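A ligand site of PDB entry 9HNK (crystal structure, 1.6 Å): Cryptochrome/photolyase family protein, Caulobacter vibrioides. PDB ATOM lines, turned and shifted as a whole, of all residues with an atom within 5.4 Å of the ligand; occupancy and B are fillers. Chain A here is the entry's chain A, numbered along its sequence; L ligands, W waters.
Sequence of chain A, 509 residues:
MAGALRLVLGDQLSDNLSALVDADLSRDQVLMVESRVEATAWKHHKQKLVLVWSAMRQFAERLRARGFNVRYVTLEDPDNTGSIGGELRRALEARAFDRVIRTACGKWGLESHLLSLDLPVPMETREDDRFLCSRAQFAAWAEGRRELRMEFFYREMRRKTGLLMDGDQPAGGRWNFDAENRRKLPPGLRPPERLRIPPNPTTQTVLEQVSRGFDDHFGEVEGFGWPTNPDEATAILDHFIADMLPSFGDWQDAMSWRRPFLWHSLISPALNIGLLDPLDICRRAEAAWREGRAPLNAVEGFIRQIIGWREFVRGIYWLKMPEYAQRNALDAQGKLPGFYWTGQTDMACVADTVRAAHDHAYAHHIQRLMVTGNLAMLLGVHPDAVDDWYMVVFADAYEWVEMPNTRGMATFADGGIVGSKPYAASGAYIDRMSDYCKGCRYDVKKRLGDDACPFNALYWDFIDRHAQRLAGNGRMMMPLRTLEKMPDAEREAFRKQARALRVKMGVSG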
ATOM      1  N   VAL A   8     -12.809  16.228  -5.462  1.00  0.00           N
ATOM      2  CA  VAL A   8     -13.637  16.074  -6.631  1.00  0.00           C
ATOM      3  C   VAL A   8     -14.930  16.823  -6.358  1.00  0.00           C
ATOM      4  O   VAL A   8     -15.673  16.452  -5.427  1.00  0.00           O
ATOM      5  CB  VAL A   8     -13.937  14.615  -6.946  1.00  0.00           C
ATOM      6  CG1 VAL A   8     -14.955  14.479  -8.053  1.00  0.00           C
ATOM      7  CG2 VAL A   8     -12.642  13.882  -7.259  1.00  0.00           C
ATOM      8  N   LEU A   9     -15.206  17.851  -7.160  1.00  0.00           N
ATOM      9  CA  LEU A   9     -16.456  18.580  -7.058  1.00  0.00           C
ATOM     10  C   LEU A   9     -17.585  18.000  -7.876  1.00  0.00           C
ATOM     11  O   LEU A   9     -17.373  17.077  -8.665  1.00  0.00           O
ATOM     12  CB  LEU A   9     -16.268  20.045  -7.336  1.00  0.00           C
ATOM     13  CG  LEU A   9     -15.140  20.793  -6.623  1.00  0.00           C
ATOM     14  CD1 LEU A   9     -14.870  22.140  -7.243  1.00  0.00           C
ATOM     15  CD2 LEU A   9     -15.502  20.889  -5.123  1.00  0.00           C
ATOM     16  N   GLY A  10     -18.808  18.530  -7.682  1.00  0.00           N
ATOM     17  CA  GLY A  10     -19.994  17.895  -8.267  1.00  0.00           C
ATOM     18  C   GLY A  10     -20.085  17.967  -9.773  1.00  0.00           C
ATOM     19  O   GLY A  10     -20.866  17.230 -10.370  1.00  0.00           O
ATOM     20  N   ASP A  11     -19.302  18.843 -10.400  1.00  0.00           N
ATOM     21  CA  ASP A  11     -19.231  18.910 -11.846  1.00  0.00           C
ATOM     22  C   ASP A  11     -17.938  18.326 -12.390  1.00  0.00           C
ATOM     23  O   ASP A  11     -17.566  18.580 -13.561  1.00  0.00           O
ATOM     24  CB  ASP A  11     -19.427  20.325 -12.408  1.00  0.00           C
ATOM     25  CG  ASP A  11     -18.419  21.313 -11.947  1.00  0.00           C
ATOM     26  OD1 ASP A  11     -17.486  21.028 -11.133  1.00  0.00           O
ATOM     27  OD2 ASP A  11     -18.454  22.405 -12.547  1.00  0.00           O
ATOM     28  N   GLN A  12     -17.273  17.482 -11.593  1.00  0.00           N
ATOM     29  CA  GLN A  12     -15.964  16.956 -11.958  1.00  0.00           C
ATOM     30  C   GLN A  12     -15.955  15.434 -11.979  1.00  0.00           C
ATOM     31  O   GLN A  12     -14.951  14.794 -11.651  1.00  0.00           O
ATOM     32  CB  GLN A  12     -14.916  17.521 -10.996  1.00  0.00           C
ATOM     33  CG  GLN A  12     -14.823  19.042 -11.052  1.00  0.00           C
ATOM     34  CD  GLN A  12     -13.686  19.585 -10.194  1.00  0.00           C
ATOM     35  OE1 GLN A  12     -13.345  18.991  -9.198  1.00  0.00           O
ATOM     36  NE2 GLN A  12     -13.168  20.730 -10.552  1.00  0.00           N
ATOM     37  N   VAL A  33     -18.103  16.060  -1.393  1.00  0.00           N
ATOM     38  CA  VAL A  33     -18.988  16.676  -0.407  1.00  0.00           C
ATOM     39  C   VAL A  33     -20.318  17.050  -1.014  1.00  0.00           C
ATOM     40  O   VAL A  33     -20.353  17.773  -2.009  1.00  0.00           O
ATOM     41  CB  VAL A  33     -18.343  17.944   0.187  1.00  0.00           C
ATOM     42  CG1 VAL A  33     -19.233  18.593   1.235  1.00  0.00           C
ATOM     43  CG2 VAL A  33     -16.954  17.628   0.748  1.00  0.00           C
ATOM     44  N   GLU A  34     -21.417  16.575  -0.427  1.00  0.00           N
ATOM     45  CA  GLU A  34     -22.720  17.136  -0.764  1.00  0.00           C
ATOM     46  C   GLU A  34     -22.881  18.411   0.063  1.00  0.00           C
ATOM     47  O   GLU A  34     -23.022  18.341   1.294  1.00  0.00           O
ATOM     48  CB  GLU A  34     -23.837  16.114  -0.490  1.00  0.00           C
ATOM     49  CG  GLU A  34     -23.662  14.856  -1.299  1.00  0.00           C
ATOM     50  CD  GLU A  34     -24.749  13.858  -1.240  1.00  0.00           C
ATOM     51  OE1 GLU A  34     -25.591  13.905  -0.322  1.00  0.00           O
ATOM     52  OE2 GLU A  34     -24.758  12.965  -2.123  1.00  0.00           O
ATOM     53  N   SER A  35     -22.801  19.560  -0.592  1.00  0.00           N
ATOM     54  CA  SER A  35     -22.607  20.845   0.064  1.00  0.00           C
ATOM     55  C   SER A  35     -23.883  21.660   0.001  1.00  0.00           C
ATOM     56  O   SER A  35     -24.321  22.032  -1.076  1.00  0.00           O
ATOM     57  CB  SER A  35     -21.445  21.584  -0.611  1.00  0.00           C
ATOM     58  OG  SER A  35     -21.337  22.898  -0.209  1.00  0.00           O
ATOM     59  N   GLU A  38     -23.177  25.008  -1.751  1.00  0.00           N
ATOM     60  CA  GLU A  38     -23.302  24.914  -3.203  1.00  0.00           C
ATOM     61  C   GLU A  38     -24.762  24.749  -3.628  1.00  0.00           C
ATOM     62  O   GLU A  38     -25.203  25.341  -4.623  1.00  0.00           O
ATOM     63  CB  GLU A  38     -22.463  23.737  -3.691  1.00  0.00           C
ATOM     64  CG  GLU A  38     -20.924  23.915  -3.598  1.00  0.00           C
ATOM     65  CD  GLU A  38     -20.441  25.338  -3.828  1.00  0.00           C
ATOM     66  OE1 GLU A  38     -20.464  25.801  -4.987  1.00  0.00           O
ATOM     67  OE2 GLU A  38     -19.905  25.969  -2.906  1.00  0.00           O
ATOM     68  N   ALA A  39     -25.551  24.015  -2.852  1.00  0.00           N
ATOM     69  CA  ALA A  39     -26.945  23.752  -3.198  1.00  0.00           C
ATOM     70  C   ALA A  39     -27.837  24.957  -3.045  1.00  0.00           C
ATOM     71  O   ALA A  39     -28.970  24.922  -3.555  1.00  0.00           O
ATOM     72  CB  ALA A  39     -27.531  22.663  -2.280  1.00  0.00           C
ATOM     73  N   HIS A  44     -31.151  26.192  -6.753  1.00  0.00           N
ATOM     74  CA  HIS A  44     -31.166  25.388  -7.975  1.00  0.00           C
ATOM     75  C   HIS A  44     -32.454  24.611  -8.144  1.00  0.00           C
ATOM     76  O   HIS A  44     -32.976  24.062  -7.178  1.00  0.00           O
ATOM     77  CB  HIS A  44     -30.060  24.381  -7.934  1.00  0.00           C
ATOM     78  CG  HIS A  44     -28.677  24.936  -7.804  1.00  0.00           C
ATOM     79  ND1 HIS A  44     -28.049  25.648  -8.784  1.00  0.00           N
ATOM     80  CD2 HIS A  44     -27.909  25.074  -6.675  1.00  0.00           C
ATOM     81  CE1 HIS A  44     -26.841  25.987  -8.367  1.00  0.00           C
ATOM     82  NE2 HIS A  44     -26.764  25.723  -7.060  1.00  0.00           N
ATOM     83  N   LYS A  48     -31.767  19.744 -10.930  1.00  0.00           N
ATOM     84  CA  LYS A  48     -30.309  19.883 -10.872  1.00  0.00           C
ATOM     85  C   LYS A  48     -29.753  19.232  -9.616  1.00  0.00           C
ATOM     86  O   LYS A  48     -28.707  18.569  -9.647  1.00  0.00           O
ATOM     87  CB  LYS A  48     -29.882  21.351 -10.966  1.00  0.00           C
ATOM     88  CG  LYS A  48     -28.493  21.498 -11.470  1.00  0.00           C
ATOM     89  CD  LYS A  48     -27.882  22.865 -11.192  1.00  0.00           C
ATOM     90  CE  LYS A  48     -28.681  23.961 -11.882  1.00  0.00           C
ATOM     91  NZ  LYS A  48     -28.021  25.319 -11.690  1.00  0.00           N
ATOM     92  N   LEU A  49     -30.434  19.427  -8.472  1.00  0.00           N
ATOM     93  CA  LEU A  49     -29.948  18.800  -7.263  1.00  0.00           C
ATOM     94  C   LEU A  49     -29.956  17.286  -7.391  1.00  0.00           C
ATOM     95  O   LEU A  49     -29.017  16.621  -6.978  1.00  0.00           O
ATOM     96  CB  LEU A  49     -30.782  19.283  -6.088  1.00  0.00           C
ATOM     97  CG  LEU A  49     -30.847  20.790  -5.784  1.00  0.00           C
ATOM     98  CD1 LEU A  49     -31.769  21.035  -4.658  1.00  0.00           C
ATOM     99  CD2 LEU A  49     -29.457  21.377  -5.511  1.00  0.00           C
ATOM    100  N   VAL A  52     -27.009  16.153  -9.814  1.00  0.00           N
ATOM    101  CA  VAL A  52     -25.660  16.252  -9.262  1.00  0.00           C
ATOM    102  C   VAL A  52     -25.445  15.238  -8.169  1.00  0.00           C
ATOM    103  O   VAL A  52     -24.472  14.500  -8.172  1.00  0.00           O
ATOM    104  CB  VAL A  52     -25.388  17.683  -8.808  1.00  0.00           C
ATOM    105  CG1 VAL A  52     -24.018  17.807  -8.185  1.00  0.00           C
ATOM    106  CG2 VAL A  52     -25.439  18.578 -10.048  1.00  0.00           C
ATOM    107  N   TRP A  53     -26.397  15.109  -7.255  1.00  0.00           N
ATOM    108  CA  TRP A  53     -26.113  14.264  -6.108  1.00  0.00           C
ATOM    109  C   TRP A  53     -26.226  12.814  -6.453  1.00  0.00           C
ATOM    110  O   TRP A  53     -25.416  12.032  -5.962  1.00  0.00           O
ATOM    111  CB  TRP A  53     -27.025  14.660  -4.945  1.00  0.00           C
ATOM    112  CG  TRP A  53     -26.620  15.952  -4.324  1.00  0.00           C
ATOM    113  CD1 TRP A  53     -25.350  16.462  -4.278  1.00  0.00           C
ATOM    114  CD2 TRP A  53     -27.469  16.897  -3.673  1.00  0.00           C
ATOM    115  NE1 TRP A  53     -25.354  17.672  -3.611  1.00  0.00           N
ATOM    116  CE2 TRP A  53     -26.637  17.958  -3.226  1.00  0.00           C
ATOM    117  CE3 TRP A  53     -28.848  16.936  -3.391  1.00  0.00           C
ATOM    118  CZ2 TRP A  53     -27.140  19.042  -2.525  1.00  0.00           C
ATOM    119  CZ3 TRP A  53     -29.374  18.063  -2.703  1.00  0.00           C
ATOM    120  CH2 TRP A  53     -28.504  19.095  -2.301  1.00  0.00           C
ATOM    121  N   MET A  56     -22.951  12.162  -8.345  1.00  0.00           N
ATOM    122  CA  MET A  56     -21.834  12.130  -7.410  1.00  0.00           C
ATOM    123  C   MET A  56     -21.766  10.810  -6.661  1.00  0.00           C
ATOM    124  O   MET A  56     -20.678  10.243  -6.491  1.00  0.00           O
ATOM    125  CB  MET A  56     -21.918  13.285  -6.371  1.00  0.00           C
ATOM    126  CG  MET A  56     -21.572  14.661  -6.921  1.00  0.00           C
ATOM    127  SD  MET A  56     -21.750  15.955  -5.651  1.00  0.00           S
ATOM    128  CE  MET A  56     -20.516  15.393  -4.485  1.00  0.00           C
ATOM    129  N   ILE A  84     -17.196  23.347   1.034  1.00  0.00           N
ATOM    130  CA  ILE A  84     -16.022  22.644   0.526  1.00  0.00           C
ATOM    131  C   ILE A  84     -14.802  22.927   1.381  1.00  0.00           C
ATOM    132  O   ILE A  84     -14.104  22.015   1.814  1.00  0.00           O
ATOM    133  CB  ILE A  84     -15.784  22.993  -0.960  1.00  0.00           C
ATOM    134  CG1 ILE A  84     -17.071  22.795  -1.755  1.00  0.00           C
ATOM    135  CG2 ILE A  84     -14.579  22.256  -1.491  1.00  0.00           C
ATOM    136  CD1 ILE A  84     -17.383  21.400  -2.011  1.00  0.00           C
ATOM    137  N   CYS A 105     -12.169  24.923 -10.660  1.00  0.00           N
ATOM    138  CA  CYS A 105     -13.603  24.696 -10.787  1.00  0.00           C
ATOM    139  C   CYS A 105     -14.229  25.676 -11.789  1.00  0.00           C
ATOM    140  O   CYS A 105     -13.543  26.434 -12.487  1.00  0.00           O
ATOM    141  CB  CYS A 105     -14.253  24.777  -9.398  1.00  0.00           C
ATOM    142  SG  CYS A 105     -14.407  26.373  -8.730  1.00  0.00           S
ATOM    143  N   GLY A 106     -15.558  25.656 -11.870  1.00  0.00           N
ATOM    144  CA  GLY A 106     -16.258  26.434 -12.868  1.00  0.00           C
ATOM    145  C   GLY A 106     -17.000  27.642 -12.350  1.00  0.00           C
ATOM    146  O   GLY A 106     -17.941  28.134 -13.011  1.00  0.00           O
ATOM    147  N   LYS A 107     -16.618  28.141 -11.172  1.00  0.00           N
ATOM    148  CA  LYS A 107     -17.242  29.320 -10.593  1.00  0.00           C
ATOM    149  C   LYS A 107     -16.114  30.172 -10.037  1.00  0.00           C
ATOM    150  O   LYS A 107     -15.358  29.711  -9.185  1.00  0.00           O
ATOM    151  CB  LYS A 107     -18.247  28.912  -9.516  1.00  0.00           C
ATOM    152  CG  LYS A 107     -18.866  30.086  -8.812  1.00  0.00           C
ATOM    153  CD  LYS A 107     -20.199  29.687  -8.154  1.00  0.00           C
ATOM    154  CE  LYS A 107     -20.003  28.473  -7.201  1.00  0.00           C
ATOM    155  NZ  LYS A 107     -21.130  28.270  -6.205  1.00  0.00           N
ATOM    156  N   LEU A 110     -15.944  30.579  -6.078  1.00  0.00           N
ATOM    157  CA  LEU A 110     -15.441  29.421  -5.348  1.00  0.00           C
ATOM    158  C   LEU A 110     -13.965  29.221  -5.629  1.00  0.00           C
ATOM    159  O   LEU A 110     -13.192  28.899  -4.722  1.00  0.00           O
ATOM    160  CB  LEU A 110     -16.258  28.184  -5.716  1.00  0.00           C
ATOM    161  CG  LEU A 110     -15.838  26.861  -5.089  1.00  0.00           C
ATOM    162  CD1 LEU A 110     -15.890  26.992  -3.580  1.00  0.00           C
ATOM    163  CD2 LEU A 110     -16.668  25.731  -5.572  1.00  0.00           C
ATOM    164  N   TYR A 398     -24.222  26.328 -14.892  1.00  0.00           N
ATOM    165  CA  TYR A 398     -23.054  26.686 -14.103  1.00  0.00           C
ATOM    166  C   TYR A 398     -22.564  28.050 -14.516  1.00  0.00           C
ATOM    167  O   TYR A 398     -22.795  28.478 -15.650  1.00  0.00           O
ATOM    168  CB  TYR A 398     -21.952  25.619 -14.259  1.00  0.00           C
ATOM    169  CG  TYR A 398     -22.470  24.262 -13.921  1.00  0.00           C
ATOM    170  CD1 TYR A 398     -23.222  23.529 -14.814  1.00  0.00           C
ATOM    171  CD2 TYR A 398     -22.387  23.798 -12.615  1.00  0.00           C
ATOM    172  CE1 TYR A 398     -23.821  22.366 -14.433  1.00  0.00           C
ATOM    173  CE2 TYR A 398     -22.964  22.616 -12.244  1.00  0.00           C
ATOM    174  CZ  TYR A 398     -23.665  21.891 -13.173  1.00  0.00           C
ATOM    175  OH  TYR A 398     -24.298  20.709 -12.747  1.00  0.00           O
HETATM  176  C1  LIG L   1     -24.396  22.493  -8.474  1.00  0.00           C
HETATM  177  C2  LIG L   1     -23.826  21.730  -7.344  1.00  0.00           C
HETATM  178  C3  LIG L   1     -24.687  21.198  -6.381  1.00  0.00           C
HETATM  179  C4  LIG L   1     -26.180  21.338  -6.423  1.00  0.00           C
HETATM  180  N1  LIG L   1     -24.199  20.519  -5.361  1.00  0.00           N
HETATM  181  C5  LIG L   1     -22.893  20.348  -5.258  1.00  0.00           C
HETATM  182  C6  LIG L   1     -22.403  19.587  -4.091  1.00  0.00           C
HETATM  183  O1  LIG L   1     -23.057  19.153  -3.270  1.00  0.00           O
HETATM  184  N2  LIG L   1     -21.074  19.435  -4.069  1.00  0.00           N
HETATM  185  C7  LIG L   1     -20.140  19.914  -5.015  1.00  0.00           C
HETATM  186  O2  LIG L   1     -18.984  19.625  -4.750  1.00  0.00           O
HETATM  187  N3  LIG L   1     -20.612  20.648  -6.067  1.00  0.00           N
HETATM  188  C8  LIG L   1     -21.949  20.832  -6.160  1.00  0.00           C
HETATM  189  N4  LIG L   1     -22.503  21.527  -7.223  1.00  0.00           N
HETATM  190  C9  LIG L   1     -21.531  22.084  -8.228  1.00  0.00           C
HETATM  191  C10 LIG L   1     -20.930  23.369  -7.628  1.00  0.00           C
HETATM  192  O3  LIG L   1     -21.897  24.133  -6.913  1.00  0.00           O
HETATM  193  C11 LIG L   1     -20.340  24.255  -8.736  1.00  0.00           C
HETATM  194  O4  LIG L   1     -21.308  24.666  -9.656  1.00  0.00           O
HETATM  195  C12 LIG L   1     -19.184  23.562  -9.484  1.00  0.00           C
HETATM  196  O5  LIG L   1     -18.291  22.909  -8.587  1.00  0.00           O
HETATM  197  C13 LIG L   1     -18.489  24.552 -10.414  1.00  0.00           C
HETATM  198  O6  LIG L   1     -17.330  23.922 -10.889  1.00  0.00           O
HETATM  199  O   HOH W   1     -23.514  26.709  -6.997  1.00  0.00           O
HETATM  200  O   HOH W   2     -17.280  17.570  -3.550  1.00  0.00           O
HETATM  201  O   HOH W   3     -21.761  27.395 -10.862  1.00  0.00           O
HETATM  202  O   HOH W   4     -15.293  22.157 -12.483  1.00  0.00           O
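Water W2 lies within hydrogen-bond range of O of Val 8, N of Val 33 and O2 of the ligand.
Water W1 lies within hydrogen-bond range of NZ of Lys 107 (3.0 Å), O3 of the ligand (3.0 Å), O of Glu 38 (3.2 Å) and NE2 of His 44 (3.4 Å).
Water W4 lies within hydrogen-bond range of the side-chain carboxylate of Asp 11, an oxygen (O6) of the ligand and the side-chain amide nitrogen of Gln 12.
OD2 of Asp 11 is in hydrogen-bond range of O6 of the ligand (2.5 Å).
N of Gly 106 is in hydrogen-bond range of O6 of the ligand (2.7 Å).
An oxygen (O1) of the ligand sits at hydrogen-bond distance from the backbone NH (N) of Ser 35 (2.7 Å).
A nitrogen (N2) of the ligand is in hydrogen-bond range of the backbone carbonyl oxygen (O) of Val 33, at 2.7 Å.
An oxygen (O1) of the ligand sits at hydrogen-bond distance from the indole nitrogen of Trp 53, at 2.8 Å.
The side-chain carboxylate of Glu 38 lies within hydrogen-bond range of an oxygen (O3) of the ligand (2.9 Å).
The backbone NH of Gly 10 is in hydrogen-bond range of an oxygen (O2) of the ligand.
Leu 9 touches the ligand (CA to O2, 3.6 Å).
Glu 34 touches the ligand.
Leu 49 touches the ligand.
Val 52 touches the ligand.
Met 56 touches the ligand.
CD1 of Ile 84 touches O2 of the ligand (3.6 Å).
CB of Cys 105 touches O6 of the ligand (3.5 Å).
Tyr 398 touches the ligand.
Hydrophobic or aromatic side chains within 4 Å of the ligand: Leu 9, Leu 49, Val 52, Trp 53, Met 56, Ile 84 and Tyr 398.
The side-chain hydroxyl (OG) of Ser 35 lies within hydrogen-bond range of the backbone NH (N) of Glu 38, at 3.2 Å.
The side-chain amino group (NZ) of Lys 107 lies within salt-bridge range of the side-chain carboxylate (OE1) of Glu 38 (2.8 Å).
O of Glu 38 is in hydrogen-bond range of NE2 of His 44 (2.9 Å).
The side-chain sulfur (SG) of Cys 105 sits at hydrogen-bond distance from the backbone carbonyl oxygen (O) of Lys 107, 3.5 Å away.
N of Leu 9 lies within hydrogen-bond range of OE1 of Gln 12 (3.0 Å).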
